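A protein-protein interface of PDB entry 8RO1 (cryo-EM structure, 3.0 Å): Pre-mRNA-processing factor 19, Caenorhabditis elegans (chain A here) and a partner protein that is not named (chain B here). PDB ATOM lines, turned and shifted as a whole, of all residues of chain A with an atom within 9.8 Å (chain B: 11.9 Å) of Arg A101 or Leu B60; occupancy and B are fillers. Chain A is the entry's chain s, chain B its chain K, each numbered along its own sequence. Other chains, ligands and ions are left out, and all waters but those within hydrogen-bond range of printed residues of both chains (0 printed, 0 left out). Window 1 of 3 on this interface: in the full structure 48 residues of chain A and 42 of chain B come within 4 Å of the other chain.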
ATOM      1  N   LEU A  93      17.507  15.690  26.883  1.00  0.00           N
ATOM      2  CA  LEU A  93      16.349  14.846  27.163  1.00  0.00           C
ATOM      3  C   LEU A  93      15.044  15.625  27.089  1.00  0.00           C
ATOM      4  O   LEU A  93      14.065  15.154  26.503  1.00  0.00           O
ATOM      5  CB  LEU A  93      16.483  14.199  28.537  1.00  0.00           C
ATOM      6  CG  LEU A  93      17.492  13.061  28.662  1.00  0.00           C
ATOM      7  CD1 LEU A  93      17.732  12.741  30.124  1.00  0.00           C
ATOM      8  CD2 LEU A  93      17.028  11.820  27.916  1.00  0.00           C
ATOM      9  N   ARG A  94      15.000  16.812  27.690  1.00  0.00           N
ATOM     10  CA  ARG A  94      13.770  17.594  27.631  1.00  0.00           C
ATOM     11  C   ARG A  94      13.492  18.117  26.228  1.00  0.00           C
ATOM     12  O   ARG A  94      12.328  18.308  25.866  1.00  0.00           O
ATOM     13  CB  ARG A  94      13.819  18.752  28.630  1.00  0.00           C
ATOM     14  CG  ARG A  94      14.982  19.720  28.496  1.00  0.00           C
ATOM     15  CD  ARG A  94      15.059  20.633  29.705  1.00  0.00           C
ATOM     16  NE  ARG A  94      13.897  21.508  29.800  1.00  0.00           N
ATOM     17  CZ  ARG A  94      13.469  22.103  30.907  1.00  0.00           C
ATOM     18  NH1 ARG A  94      12.365  22.840  30.859  1.00  0.00           N
ATOM     19  NH2 ARG A  94      14.109  21.982  32.061  1.00  0.00           N
ATOM     20  N   GLN A  95      14.527  18.363  25.427  1.00  0.00           N
ATOM     21  CA  GLN A  95      14.299  18.628  24.010  1.00  0.00           C
ATOM     22  C   GLN A  95      13.705  17.411  23.317  1.00  0.00           C
ATOM     23  O   GLN A  95      12.720  17.518  22.580  1.00  0.00           O
ATOM     24  CB  GLN A  95      15.594  19.049  23.325  1.00  0.00           C
ATOM     25  CG  GLN A  95      16.065  20.437  23.687  1.00  0.00           C
ATOM     26  CD  GLN A  95      17.141  20.933  22.744  1.00  0.00           C
ATOM     27  OE1 GLN A  95      17.934  20.148  22.224  1.00  0.00           O
ATOM     28  NE2 GLN A  95      17.167  22.240  22.506  1.00  0.00           N
ATOM     29  N   GLN A  96      14.299  16.240  23.541  1.00  0.00           N
ATOM     30  CA  GLN A  96      13.822  15.020  22.900  1.00  0.00           C
ATOM     31  C   GLN A  96      12.401  14.670  23.320  1.00  0.00           C
ATOM     32  O   GLN A  96      11.619  14.159  22.512  1.00  0.00           O
ATOM     33  CB  GLN A  96      14.759  13.863  23.228  1.00  0.00           C
ATOM     34  CG  GLN A  96      16.047  13.865  22.443  1.00  0.00           C
ATOM     35  CD  GLN A  96      16.990  12.769  22.886  1.00  0.00           C
ATOM     36  OE1 GLN A  96      16.717  12.053  23.845  1.00  0.00           O
ATOM     37  NE2 GLN A  96      18.108  12.632  22.185  1.00  0.00           N
ATOM     38  N   LEU A  97      12.044  14.933  24.574  1.00  0.00           N
ATOM     39  CA  LEU A  97      10.678  14.678  25.020  1.00  0.00           C
ATOM     40  C   LEU A  97       9.676  15.588  24.322  1.00  0.00           C
ATOM     41  O   LEU A  97       8.557  15.163  24.018  1.00  0.00           O
ATOM     42  CB  LEU A  97      10.586  14.848  26.533  1.00  0.00           C
ATOM     43  CG  LEU A  97       9.235  14.614  27.209  1.00  0.00           C
ATOM     44  CD1 LEU A  97       8.699  13.225  26.932  1.00  0.00           C
ATOM     45  CD2 LEU A  97       9.364  14.831  28.696  1.00  0.00           C
ATOM     46  N   GLN A  98      10.043  16.843  24.075  1.00  0.00           N
ATOM     47  CA  GLN A  98       9.179  17.717  23.290  1.00  0.00           C
ATOM     48  C   GLN A  98       9.042  17.228  21.855  1.00  0.00           C
ATOM     49  O   GLN A  98       7.941  17.234  21.295  1.00  0.00           O
ATOM     50  CB  GLN A  98       9.716  19.145  23.311  1.00  0.00           C
ATOM     51  CG  GLN A  98       9.557  19.846  24.648  1.00  0.00           C
ATOM     52  CD  GLN A  98      10.258  21.191  24.690  1.00  0.00           C
ATOM     53  OE1 GLN A  98      10.862  21.619  23.707  1.00  0.00           O
ATOM     54  NE2 GLN A  98      10.188  21.861  25.834  1.00  0.00           N
ATOM     55  N   ILE A  99      10.147  16.811  21.240  1.00  0.00           N
ATOM     56  CA  ILE A  99      10.104  16.320  19.864  1.00  0.00           C
ATOM     57  C   ILE A  99       9.269  15.048  19.768  1.00  0.00           C
ATOM     58  O   ILE A  99       8.482  14.882  18.830  1.00  0.00           O
ATOM     59  CB  ILE A  99      11.534  16.123  19.318  1.00  0.00           C
ATOM     60  CG1 ILE A  99      12.240  17.480  19.194  1.00  0.00           C
ATOM     61  CG2 ILE A  99      11.525  15.430  17.938  1.00  0.00           C
ATOM     62  CD1 ILE A  99      13.743  17.400  18.991  1.00  0.00           C
ATOM     63  N   ALA A 100       9.440  14.122  20.713  1.00  0.00           N
ATOM     64  CA  ALA A 100       8.679  12.875  20.667  1.00  0.00           C
ATOM     65  C   ALA A 100       7.185  13.119  20.810  1.00  0.00           C
ATOM     66  O   ALA A 100       6.382  12.519  20.089  1.00  0.00           O
ATOM     67  CB  ALA A 100       9.161  11.924  21.760  1.00  0.00           C
ATOM     68  N   ARG A 101       6.788  13.987  21.735  1.00  0.00           N
ATOM     69  CA  ARG A 101       5.373  14.305  21.884  1.00  0.00           C
ATOM     70  C   ARG A 101       4.833  15.077  20.694  1.00  0.00           C
ATOM     71  O   ARG A 101       3.655  14.942  20.353  1.00  0.00           O
ATOM     72  CB  ARG A 101       5.144  15.095  23.162  1.00  0.00           C
ATOM     73  CG  ARG A 101       5.254  14.247  24.398  1.00  0.00           C
ATOM     74  CD  ARG A 101       5.093  15.069  25.642  1.00  0.00           C
ATOM     75  NE  ARG A 101       3.717  15.541  25.779  1.00  0.00           N
ATOM     76  CZ  ARG A 101       2.851  15.203  26.729  1.00  0.00           C
ATOM     77  NH1 ARG A 101       1.641  15.752  26.722  1.00  0.00           N
ATOM     78  NH2 ARG A 101       3.161  14.358  27.700  1.00  0.00           N
ATOM     79  N   GLN A 102       5.663  15.898  20.061  1.00  0.00           N
ATOM     80  CA  GLN A 102       5.241  16.558  18.833  1.00  0.00           C
ATOM     81  C   GLN A 102       5.013  15.547  17.720  1.00  0.00           C
ATOM     82  O   GLN A 102       3.994  15.595  17.027  1.00  0.00           O
ATOM     83  CB  GLN A 102       6.280  17.601  18.422  1.00  0.00           C
ATOM     84  CG  GLN A 102       5.965  18.346  17.133  1.00  0.00           C
ATOM     85  CD  GLN A 102       6.894  19.521  16.896  1.00  0.00           C
ATOM     86  OE1 GLN A 102       7.686  19.885  17.763  1.00  0.00           O
ATOM     87  NE2 GLN A 102       6.796  20.125  15.718  1.00  0.00           N
ATOM     88  N   GLU A 103       5.961  14.634  17.518  1.00  0.00           N
ATOM     89  CA  GLU A 103       5.801  13.646  16.457  1.00  0.00           C
ATOM     90  C   GLU A 103       4.677  12.654  16.736  1.00  0.00           C
ATOM     91  O   GLU A 103       4.004  12.219  15.797  1.00  0.00           O
ATOM     92  CB  GLU A 103       7.115  12.901  16.240  1.00  0.00           C
ATOM     93  CG  GLU A 103       8.196  13.762  15.618  1.00  0.00           C
ATOM     94  CD  GLU A 103       9.388  12.955  15.151  1.00  0.00           C
ATOM     95  OE1 GLU A 103       9.663  11.897  15.753  1.00  0.00           O
ATOM     96  OE2 GLU A 103      10.058  13.383  14.188  1.00  0.00           O
ATOM     97  N   LEU A 104       4.454  12.282  17.995  1.00  0.00           N
ATOM     98  CA  LEU A 104       3.339  11.390  18.310  1.00  0.00           C
ATOM     99  C   LEU A 104       1.989  12.024  18.005  1.00  0.00           C
ATOM    100  O   LEU A 104       1.068  11.338  17.551  1.00  0.00           O
ATOM    101  CB  LEU A 104       3.401  10.971  19.775  1.00  0.00           C
ATOM    102  CG  LEU A 104       2.284  10.094  20.348  1.00  0.00           C
ATOM    103  CD1 LEU A 104       2.136   8.798  19.603  1.00  0.00           C
ATOM    104  CD2 LEU A 104       2.566   9.805  21.801  1.00  0.00           C
ATOM    105  N   SER A 105       1.831  13.316  18.289  1.00  0.00           N
ATOM    106  CA  SER A 105       0.587  13.998  17.946  1.00  0.00           C
ATOM    107  C   SER A 105       0.339  13.989  16.447  1.00  0.00           C
ATOM    108  O   SER A 105      -0.790  13.773  15.998  1.00  0.00           O
ATOM    109  CB  SER A 105       0.600  15.430  18.468  1.00  0.00           C
ATOM    110  OG  SER A 105       0.765  15.450  19.870  1.00  0.00           O
ATOM    111  N   HIS A 106       1.381  14.235  15.657  1.00  0.00           N
ATOM    112  CA  HIS A 106       1.249  14.149  14.209  1.00  0.00           C
ATOM    113  C   HIS A 106       0.952  12.726  13.762  1.00  0.00           C
ATOM    114  O   HIS A 106       0.122  12.513  12.874  1.00  0.00           O
ATOM    115  CB  HIS A 106       2.522  14.663  13.548  1.00  0.00           C
ATOM    116  CG  HIS A 106       2.462  14.682  12.056  1.00  0.00           C
ATOM    117  ND1 HIS A 106       1.725  15.614  11.359  1.00  0.00           N
ATOM    118  CD2 HIS A 106       3.045  13.890  11.126  1.00  0.00           C
ATOM    119  CE1 HIS A 106       1.855  15.395  10.063  1.00  0.00           C
ATOM    120  NE2 HIS A 106       2.651  14.355   9.894  1.00  0.00           N
ATOM    121  N   SER A 107       1.632  11.741  14.348  1.00  0.00           N
ATOM    122  CA  SER A 107       1.405  10.349  13.970  1.00  0.00           C
ATOM    123  C   SER A 107      -0.022   9.908  14.262  1.00  0.00           C
ATOM    124  O   SER A 107      -0.669   9.277  13.421  1.00  0.00           O
ATOM    125  CB  SER A 107       2.383   9.443  14.706  1.00  0.00           C
ATOM    126  OG  SER A 107       2.238   8.104  14.280  1.00  0.00           O
ATOM    127  N   LEU A 108      -0.532  10.224  15.450  1.00  0.00           N
ATOM    128  CA  LEU A 108      -1.910   9.870  15.775  1.00  0.00           C
ATOM    129  C   LEU A 108      -2.901  10.620  14.899  1.00  0.00           C
ATOM    130  O   LEU A 108      -3.961  10.088  14.559  1.00  0.00           O
ATOM    131  CB  LEU A 108      -2.190  10.149  17.249  1.00  0.00           C
ATOM    132  CG  LEU A 108      -1.503   9.220  18.252  1.00  0.00           C
ATOM    133  CD1 LEU A 108      -1.614   9.782  19.650  1.00  0.00           C
ATOM    134  CD2 LEU A 108      -2.049   7.810  18.198  1.00  0.00           C
ATOM    135  N   TYR A 109      -2.593  11.868  14.554  1.00  0.00           N
ATOM    136  CA  TYR A 109      -3.438  12.614  13.629  1.00  0.00           C
ATOM    137  C   TYR A 109      -3.512  11.931  12.275  1.00  0.00           C
ATOM    138  O   TYR A 109      -4.595  11.782  11.700  1.00  0.00           O
ATOM    139  CB  TYR A 109      -2.900  14.033  13.493  1.00  0.00           C
ATOM    140  CG  TYR A 109      -3.411  14.802  12.309  1.00  0.00           C
ATOM    141  CD1 TYR A 109      -4.756  15.007  12.111  1.00  0.00           C
ATOM    142  CD2 TYR A 109      -2.529  15.347  11.398  1.00  0.00           C
ATOM    143  CE1 TYR A 109      -5.210  15.709  11.024  1.00  0.00           C
ATOM    144  CE2 TYR A 109      -2.973  16.054  10.321  1.00  0.00           C
ATOM    145  CZ  TYR A 109      -4.310  16.234  10.135  1.00  0.00           C
ATOM    146  OH  TYR A 109      -4.729  16.958   9.049  1.00  0.00           O
ATOM    147  N   GLY A 378     -12.256  16.514  18.029  1.00  0.00           N
ATOM    148  CA  GLY A 378     -12.123  17.452  19.123  1.00  0.00           C
ATOM    149  C   GLY A 378     -12.546  16.907  20.463  1.00  0.00           C
ATOM    150  O   GLY A 378     -11.761  16.264  21.168  1.00  0.00           O
ATOM    151  N   PRO B  55      -5.844  18.542  12.728  1.00  0.00           N
ATOM    152  CA  PRO B  55      -5.360  17.914  13.967  1.00  0.00           C
ATOM    153  C   PRO B  55      -5.920  18.522  15.249  1.00  0.00           C
ATOM    154  O   PRO B  55      -5.188  18.852  16.181  1.00  0.00           O
ATOM    155  CB  PRO B  55      -3.846  18.133  13.873  1.00  0.00           C
ATOM    156  CG  PRO B  55      -3.742  19.443  13.179  1.00  0.00           C
ATOM    157  CD  PRO B  55      -4.816  19.421  12.142  1.00  0.00           C
ATOM    158  N   THR B  56      -7.235  18.647  15.302  1.00  0.00           N
ATOM    159  CA  THR B  56      -7.854  19.493  16.306  1.00  0.00           C
ATOM    160  C   THR B  56      -7.968  18.885  17.705  1.00  0.00           C
ATOM    161  O   THR B  56      -7.889  19.635  18.682  1.00  0.00           O
ATOM    162  CB  THR B  56      -9.223  19.891  15.773  1.00  0.00           C
ATOM    163  OG1 THR B  56      -9.780  18.783  15.059  1.00  0.00           O
ATOM    164  CG2 THR B  56      -9.108  21.105  14.863  1.00  0.00           C
ATOM    165  N   LYS B  57      -8.113  17.571  17.860  1.00  0.00           N
ATOM    166  CA  LYS B  57      -8.188  17.029  19.213  1.00  0.00           C
ATOM    167  C   LYS B  57      -6.803  16.905  19.827  1.00  0.00           C
ATOM    168  O   LYS B  57      -5.806  16.709  19.129  1.00  0.00           O
ATOM    169  CB  LYS B  57      -8.905  15.680  19.254  1.00  0.00           C
ATOM    170  CG  LYS B  57      -8.277  14.555  18.464  1.00  0.00           C
ATOM    171  CD  LYS B  57      -9.045  13.242  18.658  1.00  0.00           C
ATOM    172  CE  LYS B  57      -8.774  12.584  20.002  1.00  0.00           C
ATOM    173  NZ  LYS B  57      -9.492  11.288  20.137  1.00  0.00           N
ATOM    174  N   ASN B  58      -6.756  17.008  21.152  1.00  0.00           N
ATOM    175  CA  ASN B  58      -5.544  16.686  21.898  1.00  0.00           C
ATOM    176  C   ASN B  58      -5.390  15.177  21.853  1.00  0.00           C
ATOM    177  O   ASN B  58      -6.061  14.446  22.584  1.00  0.00           O
ATOM    178  CB  ASN B  58      -5.639  17.202  23.329  1.00  0.00           C
ATOM    179  CG  ASN B  58      -4.345  17.030  24.104  1.00  0.00           C
ATOM    180  OD1 ASN B  58      -3.363  16.494  23.593  1.00  0.00           O
ATOM    181  ND2 ASN B  58      -4.340  17.489  25.349  1.00  0.00           N
ATOM    182  N   TYR B  59      -4.503  14.705  20.981  1.00  0.00           N
ATOM    183  CA  TYR B  59      -4.231  13.283  20.872  1.00  0.00           C
ATOM    184  C   TYR B  59      -3.400  12.725  22.026  1.00  0.00           C
ATOM    185  O   TYR B  59      -3.288  11.500  22.134  1.00  0.00           O
ATOM    186  CB  TYR B  59      -3.519  13.040  19.546  1.00  0.00           C
ATOM    187  CG  TYR B  59      -4.429  13.190  18.351  1.00  0.00           C
ATOM    188  CD1 TYR B  59      -5.361  12.227  18.024  1.00  0.00           C
ATOM    189  CD2 TYR B  59      -4.350  14.315  17.554  1.00  0.00           C
ATOM    190  CE1 TYR B  59      -6.176  12.379  16.934  1.00  0.00           C
ATOM    191  CE2 TYR B  59      -5.159  14.474  16.471  1.00  0.00           C
ATOM    192  CZ  TYR B  59      -6.074  13.509  16.163  1.00  0.00           C
ATOM    193  OH  TYR B  59      -6.887  13.687  15.069  1.00  0.00           O
ATOM    194  N   LEU B  60      -2.836  13.574  22.889  1.00  0.00           N
ATOM    195  CA  LEU B  60      -1.899  13.162  23.932  1.00  0.00           C
ATOM    196  C   LEU B  60      -2.542  13.030  25.307  1.00  0.00           C
ATOM    197  O   LEU B  60      -1.824  12.891  26.301  1.00  0.00           O
ATOM    198  CB  LEU B  60      -0.734  14.147  24.010  1.00  0.00           C
ATOM    199  CG  LEU B  60       0.055  14.433  22.734  1.00  0.00           C
ATOM    200  CD1 LEU B  60       1.199  15.368  23.050  1.00  0.00           C
ATOM    201  CD2 LEU B  60       0.590  13.153  22.119  1.00  0.00           C
ATOM    202  N   THR B  61      -3.871  13.069  25.391  1.00  0.00           N
ATOM    203  CA  THR B  61      -4.549  13.039  26.683  1.00  0.00           C
ATOM    204  C   THR B  61      -4.371  11.721  27.432  1.00  0.00           C
ATOM    205  O   THR B  61      -4.647  11.677  28.634  1.00  0.00           O
ATOM    206  CB  THR B  61      -6.039  13.310  26.492  1.00  0.00           C
ATOM    207  OG1 THR B  61      -6.570  12.399  25.522  1.00  0.00           O
ATOM    208  CG2 THR B  61      -6.268  14.731  26.011  1.00  0.00           C
ATOM    209  N   HIS B  62      -3.921  10.656  26.766  1.00  0.00           N
ATOM    210  CA  HIS B  62      -3.556   9.437  27.481  1.00  0.00           C
ATOM    211  C   HIS B  62      -2.205   9.539  28.175  1.00  0.00           C
ATOM    212  O   HIS B  62      -1.972   8.809  29.143  1.00  0.00           O
ATOM    213  CB  HIS B  62      -3.521   8.216  26.547  1.00  0.00           C
ATOM    214  CG  HIS B  62      -2.517   8.307  25.435  1.00  0.00           C
ATOM    215  ND1 HIS B  62      -2.613   9.202  24.391  1.00  0.00           N
ATOM    216  CD2 HIS B  62      -1.379   7.605  25.219  1.00  0.00           C
ATOM    217  CE1 HIS B  62      -1.585   9.043  23.577  1.00  0.00           C
ATOM    218  NE2 HIS B  62      -0.820   8.081  24.058  1.00  0.00           N
ATOM    219  N   LEU B  63      -1.299  10.440  27.704  1.00  0.00           N
ATOM    220  CA  LEU B  63      -0.036  10.698  28.383  1.00  0.00           C
ATOM    221  C   LEU B  63      -0.225  11.814  29.409  1.00  0.00           C
ATOM    222  O   LEU B  63      -1.105  12.664  29.246  1.00  0.00           O
ATOM    223  CB  LEU B  63       1.042  11.097  27.376  1.00  0.00           C
ATOM    224  CG  LEU B  63       1.362  10.130  26.229  1.00  0.00           C
ATOM    225  CD1 LEU B  63       2.541  10.641  25.421  1.00  0.00           C
ATOM    226  CD2 LEU B  63       1.667   8.730  26.737  1.00  0.00           C
ATOM    227  N   PRO B  64       0.568  11.885  30.479  1.00  0.00           N
ATOM    228  CA  PRO B  64       0.460  13.035  31.382  1.00  0.00           C
ATOM    229  C   PRO B  64       1.019  14.310  30.770  1.00  0.00           C
ATOM    230  O   PRO B  64       1.766  14.299  29.792  1.00  0.00           O
ATOM    231  CB  PRO B  64       1.273  12.603  32.605  1.00  0.00           C
ATOM    232  CG  PRO B  64       2.252  11.643  32.075  1.00  0.00           C
ATOM    233  CD  PRO B  64       1.538  10.898  30.990  1.00  0.00           C
ATOM    234  N   VAL B  65       0.628  15.427  31.375  1.00  0.00           N
ATOM    235  CA  VAL B  65       1.268  16.716  31.091  1.00  0.00           C
ATOM    236  C   VAL B  65       2.746  16.640  31.471  1.00  0.00           C
ATOM    237  O   VAL B  65       3.078  16.067  32.528  1.00  0.00           O
ATOM    238  CB  VAL B  65       0.542  17.848  31.849  1.00  0.00           C
ATOM    239  CG1 VAL B  65       0.643  17.670  33.384  1.00  0.00           C
ATOM    240  CG2 VAL B  65       1.008  19.258  31.410  1.00  0.00           C
ATOM    241  N   PRO B  66       3.683  17.148  30.664  1.00  0.00           N
ATOM    242  CA  PRO B  66       5.097  16.989  31.015  1.00  0.00           C
ATOM    243  C   PRO B  66       5.502  17.910  32.156  1.00  0.00           C
ATOM    244  O   PRO B  66       4.860  18.922  32.444  1.00  0.00           O
ATOM    245  CB  PRO B  66       5.834  17.350  29.723  1.00  0.00           C
ATOM    246  CG  PRO B  66       4.937  18.256  29.033  1.00  0.00           C
ATOM    247  CD  PRO B  66       3.554  17.770  29.331  1.00  0.00           C
ATOM    248  N   ASP B  67       6.596  17.528  32.805  1.00  0.00           N
ATOM    249  CA  ASP B  67       6.997  18.027  34.117  1.00  0.00           C
ATOM    250  C   ASP B  67       8.490  18.329  34.101  1.00  0.00           C
ATOM    251  O   ASP B  67       9.251  17.868  34.952  1.00  0.00           O
ATOM    252  CB  ASP B  67       6.635  17.031  35.215  1.00  0.00           C
ATOM    253  CG  ASP B  67       7.221  15.654  34.970  1.00  0.00           C
ATOM    254  OD1 ASP B  67       7.731  15.410  33.856  1.00  0.00           O
ATOM    255  OD2 ASP B  67       7.169  14.813  35.892  1.00  0.00           O
ATOM    256  N   TYR B  68       8.921  19.104  33.099  1.00  0.00           N
ATOM    257  CA  TYR B  68      10.342  19.277  32.797  1.00  0.00           C
ATOM    258  C   TYR B  68      11.166  19.836  33.959  1.00  0.00           C
ATOM    259  O   TYR B  68      12.390  19.673  33.954  1.00  0.00           O
ATOM    260  CB  TYR B  68      10.545  20.189  31.575  1.00  0.00           C
ATOM    261  CG  TYR B  68       9.695  19.891  30.355  1.00  0.00           C
ATOM    262  CD1 TYR B  68      10.029  18.867  29.487  1.00  0.00           C
ATOM    263  CD2 TYR B  68       8.577  20.651  30.060  1.00  0.00           C
ATOM    264  CE1 TYR B  68       9.270  18.600  28.371  1.00  0.00           C
ATOM    265  CE2 TYR B  68       7.810  20.387  28.947  1.00  0.00           C
ATOM    266  CZ  TYR B  68       8.163  19.363  28.105  1.00  0.00           C
ATOM    267  OH  TYR B  68       7.399  19.093  26.994  1.00  0.00           O
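The backbone carbonyl oxygen (O) of Pro B64 is in hydrogen-bond range of the guanidinium group (NH2) of Arg A101, 2.5 Å away.
O of Tyr B68 lies within hydrogen-bond range of NH2 of Arg A94 (3.4 Å).
The side-chain amide oxygen (OD1) of Asn B58 sits at hydrogen-bond distance from the backbone NH (N) of Leu B60 (3.0 Å).
ND1 of His B62 sits at hydrogen-bond distance from O of Tyr B59 (3.3 Å).
The backbone carbonyl oxygen (O) of Arg A101 lies within hydrogen-bond range of the side-chain hydroxyl (OG) of Ser A105 (3.0 Å).
Among the printed residues, merely in contact across the chains: Ser A105 with Leu B60 (3.1 Å), Gln A98 with Tyr B68 (3.3 Å), Tyr A109 with Pro B55 (3.4 Å), Leu A108 with Tyr B59 (3.5 Å), Gly A378 with Lys B57 (3.5 Å), Arg A101 with Leu B60 (3.7 Å), Leu A104 with Leu B63 (3.7 Å), Arg A101 with Pro B66 (3.7 Å), Tyr A109 with Tyr B59 (3.8 Å), Leu A97 with Tyr B68 (3.8 Å), Leu A104 with Leu B60 (3.9 Å), Arg A101 with Leu B63 (3.9 Å), Ser A105 with Tyr B59 (3.9 Å) and Leu A108 with His B62 (3.996 Å).
Gln A96 touches none of the printed residues of chain B.
Leu A97 touches just one residue of chain B: Tyr B68.
Of chain B, only Leu B60, Leu B63, Pro B64 and Pro B66 come within 4 Å of Arg A101.
No residue of chain B comes within 4 Å of Gln A102.
Printed residues of chain B within 4 Å of Leu A104: Leu B60 (3.9 Å) and Leu B63 (3.7 Å).
Of the printed residues of chain B, Ser A105 touches Tyr B59 (3.9 Å) and Leu B60 (3.1 Å).
Printed residues of chain B within 4 Å of Leu A108: Tyr B59 (3.5 Å) and His B62 (3.996 Å).
Of the printed residues of chain B, Gly A378 touches Lys B57.
No residue of chain A comes within 4 Å of Asn B58.
Leu B60 touches just these residues of chain A: Arg A101 (3.7 Å), Leu A104 (3.9 Å) and Ser A105 (3.1 Å).
No residue of chain A comes within 4 Å of Thr B61.
Of chain A, only Arg A101 and Leu A104 come within 4 Å of Leu B63.
Pro B64 touches just one residue of chain A: Arg A101.
Asp B67 touches none of the printed residues of chain A.
The nearest residue of chain B that does not touch Arg A101 is Val B65 (4.4 Å).
Hydrophobic or aromatic side chains of chain B that line the printed part of chain A: Pro B55, Tyr B59, Leu B60, His B62, Leu B63, Pro B66 and Tyr B68.
Of the 18 printed residues of chain A, 9 touch a printed residue of chain B.
Printed residues of chain A that touch a printed residue of chain B: Arg A94, Leu A97, Gln A98, Arg A101, Leu A104, Ser A105, Leu A108, Tyr A109 and Gly A378.
Hydrophobic or aromatic side chains of chain A within 4 Å of the printed part of chain B: Leu A97, Leu A104, Leu A108 and Tyr A109.
Among the printed residues, 16 pairs touch across the chains.
Among the printed residues, no Asp or Glu carboxylate lies within 4 Å of a Lys or Arg side-chain nitrogen of the other chain.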
